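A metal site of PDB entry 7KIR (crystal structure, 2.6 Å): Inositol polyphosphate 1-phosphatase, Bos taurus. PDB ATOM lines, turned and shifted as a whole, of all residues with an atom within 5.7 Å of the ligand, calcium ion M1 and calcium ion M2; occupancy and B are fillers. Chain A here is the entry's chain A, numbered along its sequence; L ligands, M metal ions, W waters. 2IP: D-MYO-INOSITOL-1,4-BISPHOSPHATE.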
ATOM      1  N   LYS A  50      -4.091   4.056   2.134  1.00  0.00           N
ATOM      2  CA  LYS A  50      -4.629   3.332   3.277  1.00  0.00           C
ATOM      3  C   LYS A  50      -4.828   4.263   4.470  1.00  0.00           C
ATOM      4  O   LYS A  50      -5.900   4.270   5.102  1.00  0.00           O
ATOM      5  CB  LYS A  50      -3.741   2.129   3.624  1.00  0.00           C
ATOM      6  CG  LYS A  50      -2.350   2.451   4.207  1.00  0.00           C
ATOM      7  CD  LYS A  50      -2.006   1.559   5.393  1.00  0.00           C
ATOM      8  CE  LYS A  50      -0.958   2.167   6.301  1.00  0.00           C
ATOM      9  NZ  LYS A  50      -1.123   1.671   7.699  1.00  0.00           N
ATOM     10  N   GLU A  79      -6.659   5.579  16.630  1.00  0.00           N
ATOM     11  CA  GLU A  79      -5.315   5.261  16.162  1.00  0.00           C
ATOM     12  C   GLU A  79      -4.783   6.309  15.190  1.00  0.00           C
ATOM     13  O   GLU A  79      -3.569   6.536  15.130  1.00  0.00           O
ATOM     14  CB  GLU A  79      -5.302   3.879  15.509  1.00  0.00           C
ATOM     15  CG  GLU A  79      -3.931   3.428  15.065  1.00  0.00           C
ATOM     16  CD  GLU A  79      -3.986   2.142  14.295  1.00  0.00           C
ATOM     17  OE1 GLU A  79      -5.109   1.721  13.946  1.00  0.00           O
ATOM     18  OE2 GLU A  79      -2.912   1.549  14.041  1.00  0.00           O
ATOM     19  N   GLU A  80      -5.654   6.959  14.435  1.00  0.00           N
ATOM     20  CA  GLU A  80      -5.208   7.854  13.382  1.00  0.00           C
ATOM     21  C   GLU A  80      -5.200   9.301  13.858  1.00  0.00           C
ATOM     22  O   GLU A  80      -5.988   9.716  14.713  1.00  0.00           O
ATOM     23  CB  GLU A  80      -6.090   7.715  12.142  1.00  0.00           C
ATOM     24  CG  GLU A  80      -6.028   6.337  11.517  1.00  0.00           C
ATOM     25  CD  GLU A  80      -4.606   5.890  11.243  1.00  0.00           C
ATOM     26  OE1 GLU A  80      -3.800   6.718  10.771  1.00  0.00           O
ATOM     27  OE2 GLU A  80      -4.290   4.717  11.499  1.00  0.00           O
ATOM     28  N   ASP A 153     -10.634   2.198  16.407  1.00  0.00           N
ATOM     29  CA  ASP A 153      -9.798   1.766  15.301  1.00  0.00           C
ATOM     30  C   ASP A 153     -10.647   1.803  14.043  1.00  0.00           C
ATOM     31  O   ASP A 153     -11.544   0.955  13.887  1.00  0.00           O
ATOM     32  CB  ASP A 153      -9.241   0.365  15.538  1.00  0.00           C
ATOM     33  CG  ASP A 153      -8.122   0.038  14.577  1.00  0.00           C
ATOM     34  OD1 ASP A 153      -7.959   0.773  13.592  1.00  0.00           O
ATOM     35  OD2 ASP A 153      -7.397  -0.953  14.811  1.00  0.00           O
ATOM     36  N   PRO A 154     -10.419   2.761  13.151  1.00  0.00           N
ATOM     37  CA  PRO A 154     -11.266   2.867  11.951  1.00  0.00           C
ATOM     38  C   PRO A 154     -11.192   1.635  11.051  1.00  0.00           C
ATOM     39  O   PRO A 154     -12.230   1.189  10.550  1.00  0.00           O
ATOM     40  CB  PRO A 154     -10.736   4.125  11.264  1.00  0.00           C
ATOM     41  CG  PRO A 154      -9.356   4.328  11.840  1.00  0.00           C
ATOM     42  CD  PRO A 154      -9.422   3.834  13.230  1.00  0.00           C
ATOM     43  N   ILE A 155     -10.002   1.087  10.819  1.00  0.00           N
ATOM     44  CA  ILE A 155      -9.844  -0.120  10.015  1.00  0.00           C
ATOM     45  C   ILE A 155      -8.784  -0.994  10.669  1.00  0.00           C
ATOM     46  O   ILE A 155      -7.594  -0.651  10.646  1.00  0.00           O
ATOM     47  CB  ILE A 155      -9.448   0.174   8.554  1.00  0.00           C
ATOM     48  CG1 ILE A 155     -10.455   1.078   7.845  1.00  0.00           C
ATOM     49  CG2 ILE A 155      -9.251  -1.145   7.795  1.00  0.00           C
ATOM     50  CD1 ILE A 155      -9.934   1.659   6.545  1.00  0.00           C
ATOM     51  N   ASP A 156      -9.207  -2.110  11.235  1.00  0.00           N
ATOM     52  CA  ASP A 156      -8.269  -3.052  11.835  1.00  0.00           C
ATOM     53  C   ASP A 156      -7.918  -4.146  10.833  1.00  0.00           C
ATOM     54  O   ASP A 156      -8.757  -4.552  10.023  1.00  0.00           O
ATOM     55  CB  ASP A 156      -8.852  -3.663  13.102  1.00  0.00           C
ATOM     56  CG  ASP A 156      -7.849  -4.514  13.844  1.00  0.00           C
ATOM     57  OD1 ASP A 156      -6.801  -3.970  14.233  1.00  0.00           O
ATOM     58  OD2 ASP A 156      -8.084  -5.726  14.038  1.00  0.00           O
ATOM     59  N   SER A 157      -6.668  -4.611  10.906  1.00  0.00           N
ATOM     60  CA  SER A 157      -6.051  -5.502   9.919  1.00  0.00           C
ATOM     61  C   SER A 157      -5.959  -4.812   8.560  1.00  0.00           C
ATOM     62  O   SER A 157      -6.606  -5.172   7.576  1.00  0.00           O
ATOM     63  CB  SER A 157      -6.796  -6.839   9.814  1.00  0.00           C
ATOM     64  OG  SER A 157      -6.021  -7.792   9.117  1.00  0.00           O
ATOM     65  N   THR A 158      -5.111  -3.771   8.532  1.00  0.00           N
ATOM     66  CA  THR A 158      -4.965  -2.958   7.338  1.00  0.00           C
ATOM     67  C   THR A 158      -4.302  -3.746   6.209  1.00  0.00           C
ATOM     68  O   THR A 158      -4.613  -3.523   5.019  1.00  0.00           O
ATOM     69  CB  THR A 158      -4.154  -1.690   7.646  1.00  0.00           C
ATOM     70  OG1 THR A 158      -4.463  -1.247   8.968  1.00  0.00           O
ATOM     71  CG2 THR A 158      -4.514  -0.595   6.682  1.00  0.00           C
ATOM     72  N   TYR A 159      -3.410  -4.681   6.541  1.00  0.00           N
ATOM     73  CA  TYR A 159      -2.713  -5.446   5.520  1.00  0.00           C
ATOM     74  C   TYR A 159      -3.671  -6.401   4.799  1.00  0.00           C
ATOM     75  O   TYR A 159      -3.535  -6.639   3.598  1.00  0.00           O
ATOM     76  CB  TYR A 159      -1.542  -6.216   6.136  1.00  0.00           C
ATOM     77  CG  TYR A 159      -0.827  -7.098   5.148  1.00  0.00           C
ATOM     78  CD1 TYR A 159       0.094  -6.567   4.244  1.00  0.00           C
ATOM     79  CD2 TYR A 159      -1.064  -8.470   5.105  1.00  0.00           C
ATOM     80  CE1 TYR A 159       0.746  -7.368   3.341  1.00  0.00           C
ATOM     81  CE2 TYR A 159      -0.418  -9.285   4.200  1.00  0.00           C
ATOM     82  CZ  TYR A 159       0.493  -8.721   3.320  1.00  0.00           C
ATOM     83  OH  TYR A 159       1.139  -9.535   2.415  1.00  0.00           O
ATOM     84  N   SER A 268      -2.116 -14.823  16.631  1.00  0.00           N
ATOM     85  CA  SER A 268      -1.925 -13.951  15.481  1.00  0.00           C
ATOM     86  C   SER A 268      -0.941 -14.589  14.496  1.00  0.00           C
ATOM     87  O   SER A 268      -0.426 -15.692  14.712  1.00  0.00           O
ATOM     88  CB  SER A 268      -1.456 -12.577  15.939  1.00  0.00           C
ATOM     89  OG  SER A 268      -0.052 -12.414  15.817  1.00  0.00           O
ATOM     90  N   GLU A 269      -0.670 -13.888  13.398  1.00  0.00           N
ATOM     91  CA  GLU A 269       0.109 -14.472  12.328  1.00  0.00           C
ATOM     92  C   GLU A 269       1.604 -14.473  12.592  1.00  0.00           C
ATOM     93  O   GLU A 269       2.341 -15.237  11.956  1.00  0.00           O
ATOM     94  CB  GLU A 269      -0.174 -13.718  11.031  1.00  0.00           C
ATOM     95  CG  GLU A 269      -1.643 -13.602  10.767  1.00  0.00           C
ATOM     96  CD  GLU A 269      -1.930 -13.213   9.340  1.00  0.00           C
ATOM     97  OE1 GLU A 269      -1.125 -12.453   8.752  1.00  0.00           O
ATOM     98  OE2 GLU A 269      -2.949 -13.700   8.796  1.00  0.00           O
ATOM     99  N   LYS A 270       2.076 -13.618  13.503  1.00  0.00           N
ATOM    100  CA  LYS A 270       3.497 -13.517  13.786  1.00  0.00           C
ATOM    101  C   LYS A 270       3.807 -13.919  15.228  1.00  0.00           C
ATOM    102  O   LYS A 270       4.867 -13.567  15.755  1.00  0.00           O
ATOM    103  CB  LYS A 270       3.997 -12.101  13.507  1.00  0.00           C
ATOM    104  CG  LYS A 270       3.335 -11.044  14.364  1.00  0.00           C
ATOM    105  CD  LYS A 270       2.129 -10.450  13.668  1.00  0.00           C
ATOM    106  CE  LYS A 270       1.881  -9.009  14.086  1.00  0.00           C
ATOM    107  NZ  LYS A 270       0.811  -8.439  13.224  1.00  0.00           N
ATOM    108  N   ALA A 288      -4.803 -16.522  12.791  1.00  0.00           N
ATOM    109  CA  ALA A 288      -5.767 -15.618  12.157  1.00  0.00           C
ATOM    110  C   ALA A 288      -5.229 -14.198  12.205  1.00  0.00           C
ATOM    111  O   ALA A 288      -4.492 -13.831  13.117  1.00  0.00           O
ATOM    112  CB  ALA A 288      -7.137 -15.690  12.831  1.00  0.00           C
ATOM    113  N   ALA A 289      -5.611 -13.411  11.208  1.00  0.00           N
ATOM    114  CA  ALA A 289      -5.243 -12.005  11.141  1.00  0.00           C
ATOM    115  C   ALA A 289      -6.308 -11.148  11.813  1.00  0.00           C
ATOM    116  O   ALA A 289      -7.489 -11.502  11.833  1.00  0.00           O
ATOM    117  CB  ALA A 289      -5.066 -11.560   9.682  1.00  0.00           C
ATOM    118  N   GLY A 290      -5.863 -10.031  12.387  1.00  0.00           N
ATOM    119  CA  GLY A 290      -6.788  -9.080  12.988  1.00  0.00           C
ATOM    120  C   GLY A 290      -6.984  -9.237  14.483  1.00  0.00           C
ATOM    121  O   GLY A 290      -7.356 -10.310  14.968  1.00  0.00           O
ATOM    122  N   ALA A 291      -6.718  -8.158  15.238  1.00  0.00           N
ATOM    123  CA  ALA A 291      -7.021  -8.161  16.667  1.00  0.00           C
ATOM    124  C   ALA A 291      -8.522  -8.176  16.904  1.00  0.00           C
ATOM    125  O   ALA A 291      -9.043  -8.980  17.688  1.00  0.00           O
ATOM    126  CB  ALA A 291      -6.378  -6.955  17.339  1.00  0.00           C
ATOM    127  N   GLY A 292      -9.237  -7.285  16.202  1.00  0.00           N
ATOM    128  CA  GLY A 292     -10.684  -7.294  16.280  1.00  0.00           C
ATOM    129  C   GLY A 292     -11.277  -8.622  15.851  1.00  0.00           C
ATOM    130  O   GLY A 292     -12.166  -9.150  16.526  1.00  0.00           O
ATOM    131  N   LYS A 294      -9.905 -11.670  15.879  1.00  0.00           N
ATOM    132  CA  LYS A 294      -9.667 -12.754  16.837  1.00  0.00           C
ATOM    133  C   LYS A 294     -10.533 -12.596  18.073  1.00  0.00           C
ATOM    134  O   LYS A 294     -11.119 -13.577  18.561  1.00  0.00           O
ATOM    135  CB  LYS A 294      -8.180 -12.807  17.210  1.00  0.00           C
ATOM    136  CG  LYS A 294      -7.313 -13.429  16.114  1.00  0.00           C
ATOM    137  CD  LYS A 294      -5.862 -13.623  16.541  1.00  0.00           C
ATOM    138  CE  LYS A 294      -5.050 -12.358  16.339  1.00  0.00           C
ATOM    139  NZ  LYS A 294      -5.139 -11.883  14.927  1.00  0.00           N
ATOM    140  N   TYR A 306      -7.922 -16.169  23.272  1.00  0.00           N
ATOM    141  CA  TYR A 306      -7.107 -15.422  22.313  1.00  0.00           C
ATOM    142  C   TYR A 306      -5.921 -14.859  23.094  1.00  0.00           C
ATOM    143  O   TYR A 306      -6.095 -14.011  23.974  1.00  0.00           O
ATOM    144  CB  TYR A 306      -7.952 -14.346  21.628  1.00  0.00           C
ATOM    145  CG  TYR A 306      -7.223 -13.150  21.049  1.00  0.00           C
ATOM    146  CD1 TYR A 306      -6.040 -13.291  20.333  1.00  0.00           C
ATOM    147  CD2 TYR A 306      -7.757 -11.879  21.189  1.00  0.00           C
ATOM    148  CE1 TYR A 306      -5.387 -12.187  19.811  1.00  0.00           C
ATOM    149  CE2 TYR A 306      -7.118 -10.776  20.667  1.00  0.00           C
ATOM    150  CZ  TYR A 306      -5.941 -10.925  19.973  1.00  0.00           C
ATOM    151  OH  TYR A 306      -5.317  -9.823  19.452  1.00  0.00           O
ATOM    152  N   PHE A 308      -2.051 -13.068  23.148  1.00  0.00           N
ATOM    153  CA  PHE A 308      -1.099 -12.231  22.423  1.00  0.00           C
ATOM    154  C   PHE A 308       0.030 -11.872  23.376  1.00  0.00           C
ATOM    155  O   PHE A 308      -0.192 -11.185  24.372  1.00  0.00           O
ATOM    156  CB  PHE A 308      -1.767 -10.983  21.878  1.00  0.00           C
ATOM    157  CG  PHE A 308      -0.962 -10.289  20.828  1.00  0.00           C
ATOM    158  CD1 PHE A 308      -0.178  -9.192  21.150  1.00  0.00           C
ATOM    159  CD2 PHE A 308      -0.970 -10.759  19.523  1.00  0.00           C
ATOM    160  CE1 PHE A 308       0.570  -8.560  20.174  1.00  0.00           C
ATOM    161  CE2 PHE A 308      -0.221 -10.144  18.550  1.00  0.00           C
ATOM    162  CZ  PHE A 308       0.542  -9.044  18.867  1.00  0.00           C
ATOM    163  N   THR A 312       2.306  -5.245  20.909  1.00  0.00           N
ATOM    164  CA  THR A 312       1.963  -4.522  19.696  1.00  0.00           C
ATOM    165  C   THR A 312       0.460  -4.345  19.496  1.00  0.00           C
ATOM    166  O   THR A 312       0.028  -3.955  18.413  1.00  0.00           O
ATOM    167  CB  THR A 312       2.601  -5.208  18.491  1.00  0.00           C
ATOM    168  OG1 THR A 312       2.304  -6.613  18.533  1.00  0.00           O
ATOM    169  CG2 THR A 312       4.111  -5.025  18.527  1.00  0.00           C
ATOM    170  N   THR A 313      -0.343  -4.589  20.531  1.00  0.00           N
ATOM    171  CA  THR A 313      -1.740  -4.150  20.517  1.00  0.00           C
ATOM    172  C   THR A 313      -1.872  -2.908  21.373  1.00  0.00           C
ATOM    173  O   THR A 313      -0.985  -2.570  22.171  1.00  0.00           O
ATOM    174  CB  THR A 313      -2.707  -5.237  21.009  1.00  0.00           C
ATOM    175  OG1 THR A 313      -2.569  -5.405  22.429  1.00  0.00           O
ATOM    176  CG2 THR A 313      -2.461  -6.547  20.303  1.00  0.00           C
ATOM    177  N   PHE A 314      -2.995  -2.220  21.199  1.00  0.00           N
ATOM    178  CA  PHE A 314      -3.253  -0.946  21.871  1.00  0.00           C
ATOM    179  C   PHE A 314      -4.714  -0.909  22.313  1.00  0.00           C
ATOM    180  O   PHE A 314      -5.503  -1.797  21.979  1.00  0.00           O
ATOM    181  CB  PHE A 314      -2.940   0.251  20.957  1.00  0.00           C
ATOM    182  CG  PHE A 314      -1.611   0.157  20.263  1.00  0.00           C
ATOM    183  CD1 PHE A 314      -0.501   0.812  20.773  1.00  0.00           C
ATOM    184  CD2 PHE A 314      -1.465  -0.580  19.097  1.00  0.00           C
ATOM    185  CE1 PHE A 314       0.728   0.731  20.142  1.00  0.00           C
ATOM    186  CE2 PHE A 314      -0.242  -0.680  18.457  1.00  0.00           C
ATOM    187  CZ  PHE A 314       0.854  -0.019  18.975  1.00  0.00           C
ATOM    188  N   TRP A 316      -7.249   0.837  21.414  1.00  0.00           N
ATOM    189  CA  TRP A 316      -8.247   0.826  20.362  1.00  0.00           C
ATOM    190  C   TRP A 316      -8.399  -0.549  19.702  1.00  0.00           C
ATOM    191  O   TRP A 316      -9.441  -0.803  19.092  1.00  0.00           O
ATOM    192  CB  TRP A 316      -7.922   1.874  19.301  1.00  0.00           C
ATOM    193  CG  TRP A 316      -6.542   1.774  18.745  1.00  0.00           C
ATOM    194  CD1 TRP A 316      -6.116   0.945  17.738  1.00  0.00           C
ATOM    195  CD2 TRP A 316      -5.400   2.542  19.144  1.00  0.00           C
ATOM    196  NE1 TRP A 316      -4.773   1.139  17.494  1.00  0.00           N
ATOM    197  CE2 TRP A 316      -4.312   2.111  18.342  1.00  0.00           C
ATOM    198  CE3 TRP A 316      -5.182   3.540  20.103  1.00  0.00           C
ATOM    199  CZ2 TRP A 316      -3.034   2.666  18.469  1.00  0.00           C
ATOM    200  CZ3 TRP A 316      -3.902   4.078  20.233  1.00  0.00           C
ATOM    201  CH2 TRP A 316      -2.849   3.642  19.419  1.00  0.00           C
ATOM    202  N   ASP A 317      -7.395  -1.415  19.803  1.00  0.00           N
ATOM    203  CA  ASP A 317      -7.539  -2.782  19.280  1.00  0.00           C
ATOM    204  C   ASP A 317      -8.491  -3.597  20.126  1.00  0.00           C
ATOM    205  O   ASP A 317      -9.215  -4.455  19.596  1.00  0.00           O
ATOM    206  CB  ASP A 317      -6.183  -3.483  19.229  1.00  0.00           C
ATOM    207  CG  ASP A 317      -5.331  -3.016  18.071  1.00  0.00           C
ATOM    208  OD1 ASP A 317      -5.902  -2.729  17.009  1.00  0.00           O
ATOM    209  OD2 ASP A 317      -4.092  -2.950  18.218  1.00  0.00           O
HETATM  210  C1  2IP L   1      -2.701  -4.352  13.868  1.00  0.00           C
HETATM  211  C2  2IP L   1      -3.851  -5.315  13.694  1.00  0.00           C
HETATM  212  C3  2IP L   1      -3.160  -6.601  13.525  1.00  0.00           C
HETATM  213  C4  2IP L   1      -2.391  -7.094  14.711  1.00  0.00           C
HETATM  214  C5  2IP L   1      -1.341  -6.033  15.020  1.00  0.00           C
HETATM  215  C6  2IP L   1      -2.048  -4.722  15.177  1.00  0.00           C
HETATM  216  O1  2IP L   1      -3.243  -3.092  13.789  1.00  0.00           O
HETATM  217  O2  2IP L   1      -4.606  -5.450  14.851  1.00  0.00           O
HETATM  218  O3  2IP L   1      -4.215  -7.447  13.227  1.00  0.00           O
HETATM  219  O4  2IP L   1      -1.646  -8.149  14.314  1.00  0.00           O
HETATM  220  O5  2IP L   1      -0.642  -6.461  16.149  1.00  0.00           O
HETATM  221  O6  2IP L   1      -1.036  -3.803  15.440  1.00  0.00           O
HETATM  222  P4  2IP L   1      -2.319  -9.601  13.960  1.00  0.00           P
HETATM  223  O41 2IP L   1      -3.395  -9.989  14.920  1.00  0.00           O
HETATM  224  O42 2IP L   1      -1.042 -10.549  13.754  1.00  0.00           O
HETATM  225  O43 2IP L   1      -2.958  -9.482  12.493  1.00  0.00           O
HETATM  226  P1  2IP L   1      -3.494  -2.484  12.315  1.00  0.00           P
HETATM  227  O11 2IP L   1      -4.711  -1.567  12.544  1.00  0.00           O
HETATM  228  O12 2IP L   1      -3.992  -3.445  11.352  1.00  0.00           O
HETATM  229  O13 2IP L   1      -2.231  -1.684  11.809  1.00  0.00           O
HETATM  230 CA    CA M   1      -5.923   0.375  12.180  1.00  0.00          CA
HETATM  231 CA    CA M   2      -5.280  -2.211  14.772  1.00  0.00          CA
HETATM  232  O   HOH W   1      -2.296  -4.649   9.759  1.00  0.00           O
HETATM  233  O   HOH W   2      -5.958   2.599  10.771  1.00  0.00           O
HETATM  234  O   HOH W   3      -3.715  -7.646  10.735  1.00  0.00           O
HETATM  235  O   HOH W   4      -2.794  -0.913  15.824  1.00  0.00           O
HETATM  236  O   HOH W   5      -3.370   0.683  11.220  1.00  0.00           O
HETATM  237  O   HOH W   6      -3.237  -9.963  17.653  1.00  0.00           O
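An oxygen (O42) of the ligand sits at hydrogen-bond distance from the backbone NH of Glu 269, at 3.4 Å. An oxygen (O43) of the ligand lies within hydrogen-bond range of the backbone NH (N) of Gly 290 (3.0 Å). The side-chain amino group (NZ) of Lys 294 is in salt-bridge range of an oxygen (O41) of the ligand. An oxygen (O12) of the ligand lies within hydrogen-bond range of the backbone NH (N) of Ser 157. The side-chain amino group (NZ) of Lys 270 lies within salt-bridge range of an oxygen (O42) of the ligand, at 2.9 Å. O42 of the ligand is in hydrogen-bond range of OG of Ser 268 (3.0 Å). An oxygen (O6) of the ligand lies within hydrogen-bond range of the backbone carbonyl oxygen (O) of Thr 312. OG1 of Thr 158 is in hydrogen-bond range of O12 of the ligand. The backbone NH (N) of Ala 291 is in hydrogen-bond range of an oxygen (O3) of the ligand (3.3 Å). An oxygen (O12) of the ligand is in hydrogen-bond range of the backbone NH of Thr 158 (3.1 Å).
OD2 of Asp 156 lies within hydrogen-bond range of N of Ala 291 (3.0 Å). The side-chain hydroxyl (OG) of Ser 268 sits close to the backbone NH (N) of Lys 270 (3.4 Å). The backbone NH of Phe 314 lies within hydrogen-bond range of the side-chain carboxylate of Asp 317. OD2 of Asp 156 sits at hydrogen-bond distance from N of Gly 292, at 2.9 Å. The side-chain amino group (NZ) of Lys 294 sits at hydrogen-bond distance from the backbone carbonyl oxygen (O) of Ala 288 (2.7 Å). The side-chain amino group of Lys 294 sits at hydrogen-bond distance from the backbone carbonyl oxygen of Gly 290 (2.7 Å).
Ala 289 touches the ligand. Phe 308 touches the ligand (CZ to O5, 3.9 Å). 16 residues have an atom within 4 Å of the ligand: Glu 79, Asp 153, Ile 155, Asp 156, Ser 157, Thr 158, Ser 268, Glu 269, Lys 270, Ala 289, Gly 290, Ala 291, Lys 294, Phe 308, Thr 312 and Asp 317. Along chain A the residues within 4 Å of the ligand span positions 79 to 317.
Residues that only touch calcium ion M1: Thr 158. Four residues have an atom within 4 Å of calcium ion M1: Glu 79, Asp 153, Ile 155 and Thr 158. The nearest printed residue that does not touch calcium ion M1 is Asp 156 (4.2 Å).
Three residues have an atom within 4 Å of calcium ion M2: Asp 153, Asp 156 and Asp 317.
Calcium ion M1 is bound by an oxygen (O11) of the ligand, the side-chain carboxylate (OE1) of Glu 79, the backbone carbonyl oxygen (O) of Ile 155, the side-chain carboxylate (OD1) of Asp 153, water W2 and water W5. Calcium ion M1 has six donor atoms within binding distance.
Calcium ion M2 is bound by OD1 of Asp 317 (2.4 Å), OD1 of Asp 156 (2.4 Å), O11 of the ligand (2.4 Å), O1 of the ligand (2.4 Å) and OD2 of Asp 153 (2.5 Å). Slightly farther from calcium ion M2 lies water W4 (3.0 Å).
Water W5 lies within hydrogen-bond range of O13 of the ligand (2.7 Å), OE2 of Glu 79 (3.0 Å) and OG1 of Thr 158 (3.2 Å). Water W4 lies within hydrogen-bond range of OE2 of Glu 79 (3.0 Å), NE1 of Trp 316 (3.3 Å), OD2 of Asp 317 (3.4 Å) and O6 of the ligand (3.4 Å). Water W3 bridges O3 of the ligand (2.5 Å) and OG of Ser 157 (2.8 Å). Water W1 lies within hydrogen-bond range of an oxygen (O12) of the ligand (2.6 Å), the backbone NH of Thr 158 (3.2 Å) and the backbone NH of Tyr 159 (3.4 Å). Water W6 lies within hydrogen-bond range of O41 of the ligand (2.7 Å) and OH of Tyr 306 (2.8 Å).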
